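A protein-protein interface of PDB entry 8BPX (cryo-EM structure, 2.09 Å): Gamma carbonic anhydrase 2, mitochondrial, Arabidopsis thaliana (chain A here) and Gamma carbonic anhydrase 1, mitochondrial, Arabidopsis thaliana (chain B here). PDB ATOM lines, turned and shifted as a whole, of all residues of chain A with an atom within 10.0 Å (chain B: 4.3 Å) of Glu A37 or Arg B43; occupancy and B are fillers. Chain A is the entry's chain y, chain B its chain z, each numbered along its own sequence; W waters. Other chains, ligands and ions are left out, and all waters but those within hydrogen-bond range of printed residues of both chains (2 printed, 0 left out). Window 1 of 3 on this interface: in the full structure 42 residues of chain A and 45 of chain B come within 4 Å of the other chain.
The guanidinium group (NH1) of Arg B43 is in hydrogen-bond range of the backbone carbonyl oxygen (O) of Ile A35 (3.0 Å).
N of Ile A35 is in hydrogen-bond range of OD1 of Asn B47, at 2.9 Å.
The guanidinium group (NH2) of Arg B41 is in salt-bridge range of the side-chain carboxylate (OE1) of Glu A37 (2.9 Å).
The guanidinium group (NH2) of Arg A34 lies within salt-bridge range of the side-chain carboxylate (OE1) of Glu A37 (3.0 Å).
SD of Met B46 sits close to NH2 of Arg B43.
Among the printed residues, merely in contact across the chains: Arg A34 with Asn B47, His A33 with Asn B47, Ile A35 with Leu B45, Arg A34 with Arg B43 and Glu A37 with Arg B43.
Printed residues of chain B within 4 Å of Glu A37: Arg B41 and Arg B43.
Of chain A, only Arg A34, Ile A35 and Glu A37 come within 4 Å of Arg B43.
Arg B41 touches just one residue of chain A: Glu A37.
No residue of chain A comes within 4 Å of Thr B44.
Printed residues of chain A within 4 Å of Leu B45: Ile A35 (3.5 Å).
Of the printed residues of chain B, Ile A35 touches Arg B43, Leu B45 and Asn B47.
Of the printed residues of chain B, His A33 touches Asn B47 (3.5 Å).
Of the printed residues of chain B, Arg A34 touches Arg B43 (3.8 Å) and Asn B47 (3.4 Å).
Ser A40 touches none of the printed residues of chain B.
The nearest residue of chain A that does not touch Arg B43 is Glu A36 (4.1 Å).
Of the 13 printed residues of chain A, 4 touch a printed residue of chain B.
Hydrophobic or aromatic side chains of chain A within 4 Å of the printed part of chain B: Ile A35.
Among the printed residues, 8 pairs touch across the chains.
Among the printed residues, Asp or Glu carboxylates within 4 Å of a Lys or Arg side-chain nitrogen of the other chain: Glu A37 with Arg B41 (2.9 Å).
Water W1 lies within hydrogen-bond range of O of His B42 and O of His A38.
Water W2 lies within hydrogen-bond range of NH2 of Arg A34 (3.3 Å) and NH2 of Arg B41 (3.4 Å).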
ATOM      1  N   ASP A  23     -32.775  -4.679 -17.178  1.00  0.00           N
ATOM      2  CA  ASP A  23     -31.593  -4.533 -16.335  1.00  0.00           C
ATOM      3  C   ASP A  23     -31.829  -5.128 -14.951  1.00  0.00           C
ATOM      4  O   ASP A  23     -30.953  -5.808 -14.402  1.00  0.00           O
ATOM      5  CB  ASP A  23     -31.194  -3.059 -16.232  1.00  0.00           C
ATOM      6  CG  ASP A  23     -29.775  -2.865 -15.717  1.00  0.00           C
ATOM      7  OD1 ASP A  23     -28.925  -3.750 -15.933  1.00  0.00           O
ATOM      8  OD2 ASP A  23     -29.506  -1.819 -15.090  1.00  0.00           O
ATOM      9  N   SER A  27     -29.849  -8.251 -13.258  1.00  0.00           N
ATOM     10  CA  SER A  27     -29.243  -8.162 -11.935  1.00  0.00           C
ATOM     11  C   SER A  27     -29.700  -9.310 -11.042  1.00  0.00           C
ATOM     12  O   SER A  27     -28.898  -9.881 -10.295  1.00  0.00           O
ATOM     13  CB  SER A  27     -29.572  -6.818 -11.293  1.00  0.00           C
ATOM     14  OG  SER A  27     -29.077  -5.747 -12.075  1.00  0.00           O
ATOM     15  N   GLN A  30     -27.856 -12.498 -11.778  1.00  0.00           N
ATOM     16  CA  GLN A  30     -26.443 -12.505 -11.309  1.00  0.00           C
ATOM     17  C   GLN A  30     -26.390 -12.802  -9.804  1.00  0.00           C
ATOM     18  O   GLN A  30     -25.330 -12.701  -9.220  1.00  0.00           O
ATOM     19  CB  GLN A  30     -25.778 -11.157 -11.584  1.00  0.00           C
ATOM     20  CG  GLN A  30     -25.583 -10.768 -13.032  1.00  0.00           C
ATOM     21  CD  GLN A  30     -24.744  -9.516 -13.118  1.00  0.00           C
ATOM     22  OE1 GLN A  30     -24.948  -8.556 -12.389  1.00  0.00           O
ATOM     23  NE2 GLN A  30     -23.762  -9.537 -13.998  1.00  0.00           N
ATOM     24  N   SER A  32     -27.557 -11.020  -7.517  1.00  0.00           N
ATOM     25  CA  SER A  32     -27.425  -9.735  -6.834  1.00  0.00           C
ATOM     26  C   SER A  32     -26.035  -9.532  -6.241  1.00  0.00           C
ATOM     27  O   SER A  32     -25.870  -8.769  -5.288  1.00  0.00           O
ATOM     28  CB  SER A  32     -28.492  -9.575  -5.749  1.00  0.00           C
ATOM     29  OG  SER A  32     -29.689  -9.053  -6.292  1.00  0.00           O
ATOM     30  N   HIS A  33     -25.024 -10.205  -6.794  1.00  0.00           N
ATOM     31  CA  HIS A  33     -23.683 -10.129  -6.232  1.00  0.00           C
ATOM     32  C   HIS A  33     -22.980  -8.824  -6.577  1.00  0.00           C
ATOM     33  O   HIS A  33     -22.170  -8.337  -5.781  1.00  0.00           O
ATOM     34  CB  HIS A  33     -22.843 -11.311  -6.716  1.00  0.00           C
ATOM     35  CG  HIS A  33     -23.181 -12.603  -6.044  1.00  0.00           C
ATOM     36  ND1 HIS A  33     -23.918 -12.663  -4.881  1.00  0.00           N
ATOM     37  CD2 HIS A  33     -22.882 -13.882  -6.368  1.00  0.00           C
ATOM     38  CE1 HIS A  33     -24.062 -13.926  -4.521  1.00  0.00           C
ATOM     39  NE2 HIS A  33     -23.440 -14.685  -5.404  1.00  0.00           N
ATOM     40  N   ARG A  34     -23.335  -8.224  -7.710  1.00  0.00           N
ATOM     41  CA  ARG A  34     -22.651  -7.016  -8.203  1.00  0.00           C
ATOM     42  C   ARG A  34     -23.000  -5.810  -7.361  1.00  0.00           C
ATOM     43  O   ARG A  34     -24.144  -5.390  -7.434  1.00  0.00           O
ATOM     44  CB  ARG A  34     -22.860  -6.813  -9.704  1.00  0.00           C
ATOM     45  CG  ARG A  34     -21.844  -5.821 -10.251  1.00  0.00           C
ATOM     46  CD  ARG A  34     -22.092  -5.316 -11.654  1.00  0.00           C
ATOM     47  NE  ARG A  34     -21.015  -4.472 -12.156  1.00  0.00           N
ATOM     48  CZ  ARG A  34     -20.977  -3.150 -12.077  1.00  0.00           C
ATOM     49  NH1 ARG A  34     -21.962  -2.489 -11.496  1.00  0.00           N
ATOM     50  NH2 ARG A  34     -19.938  -2.490 -12.552  1.00  0.00           N
ATOM     51  N   ILE A  35     -22.013  -5.264  -6.651  1.00  0.00           N
ATOM     52  CA  ILE A  35     -22.260  -4.006  -5.963  1.00  0.00           C
ATOM     53  C   ILE A  35     -22.457  -2.908  -7.001  1.00  0.00           C
ATOM     54  O   ILE A  35     -21.661  -2.765  -7.937  1.00  0.00           O
ATOM     55  CB  ILE A  35     -21.104  -3.683  -5.006  1.00  0.00           C
ATOM     56  CG1 ILE A  35     -21.026  -4.735  -3.893  1.00  0.00           C
ATOM     57  CG2 ILE A  35     -21.264  -2.290  -4.425  1.00  0.00           C
ATOM     58  CD1 ILE A  35     -19.767  -4.670  -3.074  1.00  0.00           C
ATOM     59  N   GLU A  36     -23.523  -2.132  -6.845  1.00  0.00           N
ATOM     60  CA  GLU A  36     -23.873  -1.130  -7.841  1.00  0.00           C
ATOM     61  C   GLU A  36     -23.000   0.112  -7.717  1.00  0.00           C
ATOM     62  O   GLU A  36     -22.679   0.561  -6.614  1.00  0.00           O
ATOM     63  CB  GLU A  36     -25.344  -0.739  -7.714  1.00  0.00           C
ATOM     64  CG  GLU A  36     -26.306  -1.862  -8.021  1.00  0.00           C
ATOM     65  CD  GLU A  36     -27.598  -1.360  -8.638  1.00  0.00           C
ATOM     66  OE1 GLU A  36     -28.241  -0.478  -8.032  1.00  0.00           O
ATOM     67  OE2 GLU A  36     -27.966  -1.843  -9.729  1.00  0.00           O
ATOM     68  N   GLU A  37     -22.612   0.656  -8.865  1.00  0.00           N
ATOM     69  CA  GLU A  37     -21.981   1.964  -8.905  1.00  0.00           C
ATOM     70  C   GLU A  37     -22.977   3.028  -8.452  1.00  0.00           C
ATOM     71  O   GLU A  37     -24.185   2.907  -8.665  1.00  0.00           O
ATOM     72  CB  GLU A  37     -21.485   2.251 -10.322  1.00  0.00           C
ATOM     73  CG  GLU A  37     -20.486   1.225 -10.845  1.00  0.00           C
ATOM     74  CD  GLU A  37     -20.159   1.428 -12.304  1.00  0.00           C
ATOM     75  OE1 GLU A  37     -20.326   0.476 -13.089  1.00  0.00           O
ATOM     76  OE2 GLU A  37     -19.770   2.552 -12.674  1.00  0.00           O
ATOM     77  N   HIS A  38     -22.467   4.078  -7.814  1.00  0.00           N
ATOM     78  CA  HIS A  38     -23.330   5.096  -7.229  1.00  0.00           C
ATOM     79  C   HIS A  38     -22.758   6.484  -7.484  1.00  0.00           C
ATOM     80  O   HIS A  38     -21.650   6.644  -8.000  1.00  0.00           O
ATOM     81  CB  HIS A  38     -23.528   4.868  -5.726  1.00  0.00           C
ATOM     82  CG  HIS A  38     -24.214   3.581  -5.396  1.00  0.00           C
ATOM     83  ND1 HIS A  38     -25.446   3.242  -5.912  1.00  0.00           N
ATOM     84  CD2 HIS A  38     -23.841   2.549  -4.603  1.00  0.00           C
ATOM     85  CE1 HIS A  38     -25.801   2.054  -5.453  1.00  0.00           C
ATOM     86  NE2 HIS A  38     -24.845   1.613  -4.655  1.00  0.00           N
ATOM     87  N   LEU A  39     -23.545   7.492  -7.117  1.00  0.00           N
ATOM     88  CA  LEU A  39     -23.095   8.875  -7.189  1.00  0.00           C
ATOM     89  C   LEU A  39     -21.850   9.070  -6.331  1.00  0.00           C
ATOM     90  O   LEU A  39     -21.745   8.526  -5.230  1.00  0.00           O
ATOM     91  CB  LEU A  39     -24.208   9.809  -6.721  1.00  0.00           C
ATOM     92  CG  LEU A  39     -24.226  11.222  -7.294  1.00  0.00           C
ATOM     93  CD1 LEU A  39     -24.177  11.190  -8.809  1.00  0.00           C
ATOM     94  CD2 LEU A  39     -25.448  11.964  -6.801  1.00  0.00           C
ATOM     95  N   SER A  40     -20.904   9.853  -6.843  1.00  0.00           N
ATOM     96  CA  SER A  40     -19.639  10.039  -6.145  1.00  0.00           C
ATOM     97  C   SER A  40     -19.854  10.779  -4.830  1.00  0.00           C
ATOM     98  O   SER A  40     -20.479  11.842  -4.795  1.00  0.00           O
ATOM     99  CB  SER A  40     -18.649  10.801  -7.024  1.00  0.00           C
ATOM    100  OG  SER A  40     -17.425  11.009  -6.342  1.00  0.00           O
ATOM    101  N   ARG A  41     -19.326  10.211  -3.750  1.00  0.00           N
ATOM    102  CA  ARG A  41     -19.419  10.806  -2.426  1.00  0.00           C
ATOM    103  C   ARG A  41     -18.118  11.458  -1.976  1.00  0.00           C
ATOM    104  O   ARG A  41     -18.048  11.953  -0.849  1.00  0.00           O
ATOM    105  CB  ARG A  41     -19.853   9.748  -1.405  1.00  0.00           C
ATOM    106  CG  ARG A  41     -21.263   9.216  -1.638  1.00  0.00           C
ATOM    107  CD  ARG A  41     -21.839   8.566  -0.392  1.00  0.00           C
ATOM    108  NE  ARG A  41     -21.933   9.500   0.723  1.00  0.00           N
ATOM    109  CZ  ARG A  41     -23.038  10.146   1.072  1.00  0.00           C
ATOM    110  NH1 ARG A  41     -24.172   9.981   0.413  1.00  0.00           N
ATOM    111  NH2 ARG A  41     -23.001  10.983   2.104  1.00  0.00           N
ATOM    112  N   ARG B  41     -16.661   5.748 -12.150  1.00  0.00           N
ATOM    113  CA  ARG B  41     -17.124   4.397 -11.888  1.00  0.00           C
ATOM    114  C   ARG B  41     -16.443   3.782 -10.674  1.00  0.00           C
ATOM    115  O   ARG B  41     -16.530   2.569 -10.470  1.00  0.00           O
ATOM    116  CB  ARG B  41     -16.919   3.531 -13.131  1.00  0.00           C
ATOM    117  CG  ARG B  41     -17.391   4.226 -14.405  1.00  0.00           C
ATOM    118  CD  ARG B  41     -17.521   3.282 -15.586  1.00  0.00           C
ATOM    119  NE  ARG B  41     -18.468   2.199 -15.346  1.00  0.00           N
ATOM    120  CZ  ARG B  41     -18.869   1.341 -16.276  1.00  0.00           C
ATOM    121  NH1 ARG B  41     -18.435   1.423 -17.523  1.00  0.00           N
ATOM    122  NH2 ARG B  41     -19.721   0.376 -15.946  1.00  0.00           N
ATOM    123  N   HIS B  42     -15.760   4.596  -9.874  1.00  0.00           N
ATOM    124  CA  HIS B  42     -15.129   4.106  -8.660  1.00  0.00           C
ATOM    125  C   HIS B  42     -16.173   3.574  -7.690  1.00  0.00           C
ATOM    126  O   HIS B  42     -17.193   4.217  -7.441  1.00  0.00           O
ATOM    127  CB  HIS B  42     -14.325   5.218  -7.991  1.00  0.00           C
ATOM    128  CG  HIS B  42     -13.930   4.901  -6.582  1.00  0.00           C
ATOM    129  ND1 HIS B  42     -12.941   3.993  -6.275  1.00  0.00           N
ATOM    130  CD2 HIS B  42     -14.400   5.359  -5.398  1.00  0.00           C
ATOM    131  CE1 HIS B  42     -12.811   3.911  -4.963  1.00  0.00           C
ATOM    132  NE2 HIS B  42     -13.687   4.729  -4.407  1.00  0.00           N
ATOM    133  N   ARG B  43     -15.906   2.398  -7.138  1.00  0.00           N
ATOM    134  CA  ARG B  43     -16.720   1.812  -6.086  1.00  0.00           C
ATOM    135  C   ARG B  43     -15.850   1.637  -4.852  1.00  0.00           C
ATOM    136  O   ARG B  43     -14.770   1.045  -4.931  1.00  0.00           O
ATOM    137  CB  ARG B  43     -17.312   0.470  -6.530  1.00  0.00           C
ATOM    138  CG  ARG B  43     -18.554   0.604  -7.406  1.00  0.00           C
ATOM    139  CD  ARG B  43     -19.013  -0.741  -7.950  1.00  0.00           C
ATOM    140  NE  ARG B  43     -18.051  -1.312  -8.883  1.00  0.00           N
ATOM    141  CZ  ARG B  43     -18.013  -2.588  -9.243  1.00  0.00           C
ATOM    142  NH1 ARG B  43     -18.888  -3.466  -8.779  1.00  0.00           N
ATOM    143  NH2 ARG B  43     -17.082  -2.991 -10.103  1.00  0.00           N
ATOM    144  N   THR B  44     -16.311   2.167  -3.720  1.00  0.00           N
ATOM    145  CA  THR B  44     -15.558   2.014  -2.479  1.00  0.00           C
ATOM    146  C   THR B  44     -15.410   0.545  -2.112  1.00  0.00           C
ATOM    147  O   THR B  44     -14.327   0.100  -1.715  1.00  0.00           O
ATOM    148  CB  THR B  44     -16.245   2.788  -1.353  1.00  0.00           C
ATOM    149  OG1 THR B  44     -16.434   4.150  -1.752  1.00  0.00           O
ATOM    150  CG2 THR B  44     -15.408   2.750  -0.093  1.00  0.00           C
ATOM    151  N   LEU B  45     -16.484  -0.224  -2.250  1.00  0.00           N
ATOM    152  CA  LEU B  45     -16.450  -1.671  -2.112  1.00  0.00           C
ATOM    153  C   LEU B  45     -16.724  -2.292  -3.473  1.00  0.00           C
ATOM    154  O   LEU B  45     -17.740  -1.985  -4.103  1.00  0.00           O
ATOM    155  CB  LEU B  45     -17.479  -2.153  -1.089  1.00  0.00           C
ATOM    156  CG  LEU B  45     -17.491  -1.436   0.262  1.00  0.00           C
ATOM    157  CD1 LEU B  45     -18.534  -2.057   1.178  1.00  0.00           C
ATOM    158  CD2 LEU B  45     -16.110  -1.465   0.911  1.00  0.00           C
ATOM    159  N   MET B  46     -15.826  -3.163  -3.918  1.00  0.00           N
ATOM    160  CA  MET B  46     -15.931  -3.787  -5.229  1.00  0.00           C
ATOM    161  C   MET B  46     -15.864  -5.296  -5.091  1.00  0.00           C
ATOM    162  O   MET B  46     -14.958  -5.825  -4.439  1.00  0.00           O
ATOM    163  CB  MET B  46     -14.824  -3.304  -6.170  1.00  0.00           C
ATOM    164  CG  MET B  46     -15.046  -3.713  -7.612  1.00  0.00           C
ATOM    165  SD  MET B  46     -13.778  -3.116  -8.743  1.00  0.00           S
ATOM    166  CE  MET B  46     -13.795  -4.420  -9.972  1.00  0.00           C
ATOM    167  N   ASN B  47     -16.804  -5.983  -5.727  1.00  0.00           N
ATOM    168  CA  ASN B  47     -16.809  -7.432  -5.773  1.00  0.00           C
ATOM    169  C   ASN B  47     -16.105  -7.928  -7.029  1.00  0.00           C
ATOM    170  O   ASN B  47     -16.117  -7.276  -8.077  1.00  0.00           O
ATOM    171  CB  ASN B  47     -18.241  -7.967  -5.743  1.00  0.00           C
ATOM    172  CG  ASN B  47     -19.007  -7.643  -7.009  1.00  0.00           C
ATOM    173  OD1 ASN B  47     -19.494  -6.529  -7.181  1.00  0.00           O
ATOM    174  ND2 ASN B  47     -19.106  -8.613  -7.907  1.00  0.00           N
HETATM  175  O   HOH W   1     -19.305   4.428  -9.098  1.00  0.00           O
HETATM  176  O   HOH W   2     -21.095  -2.702 -15.592  1.00  0.00           O
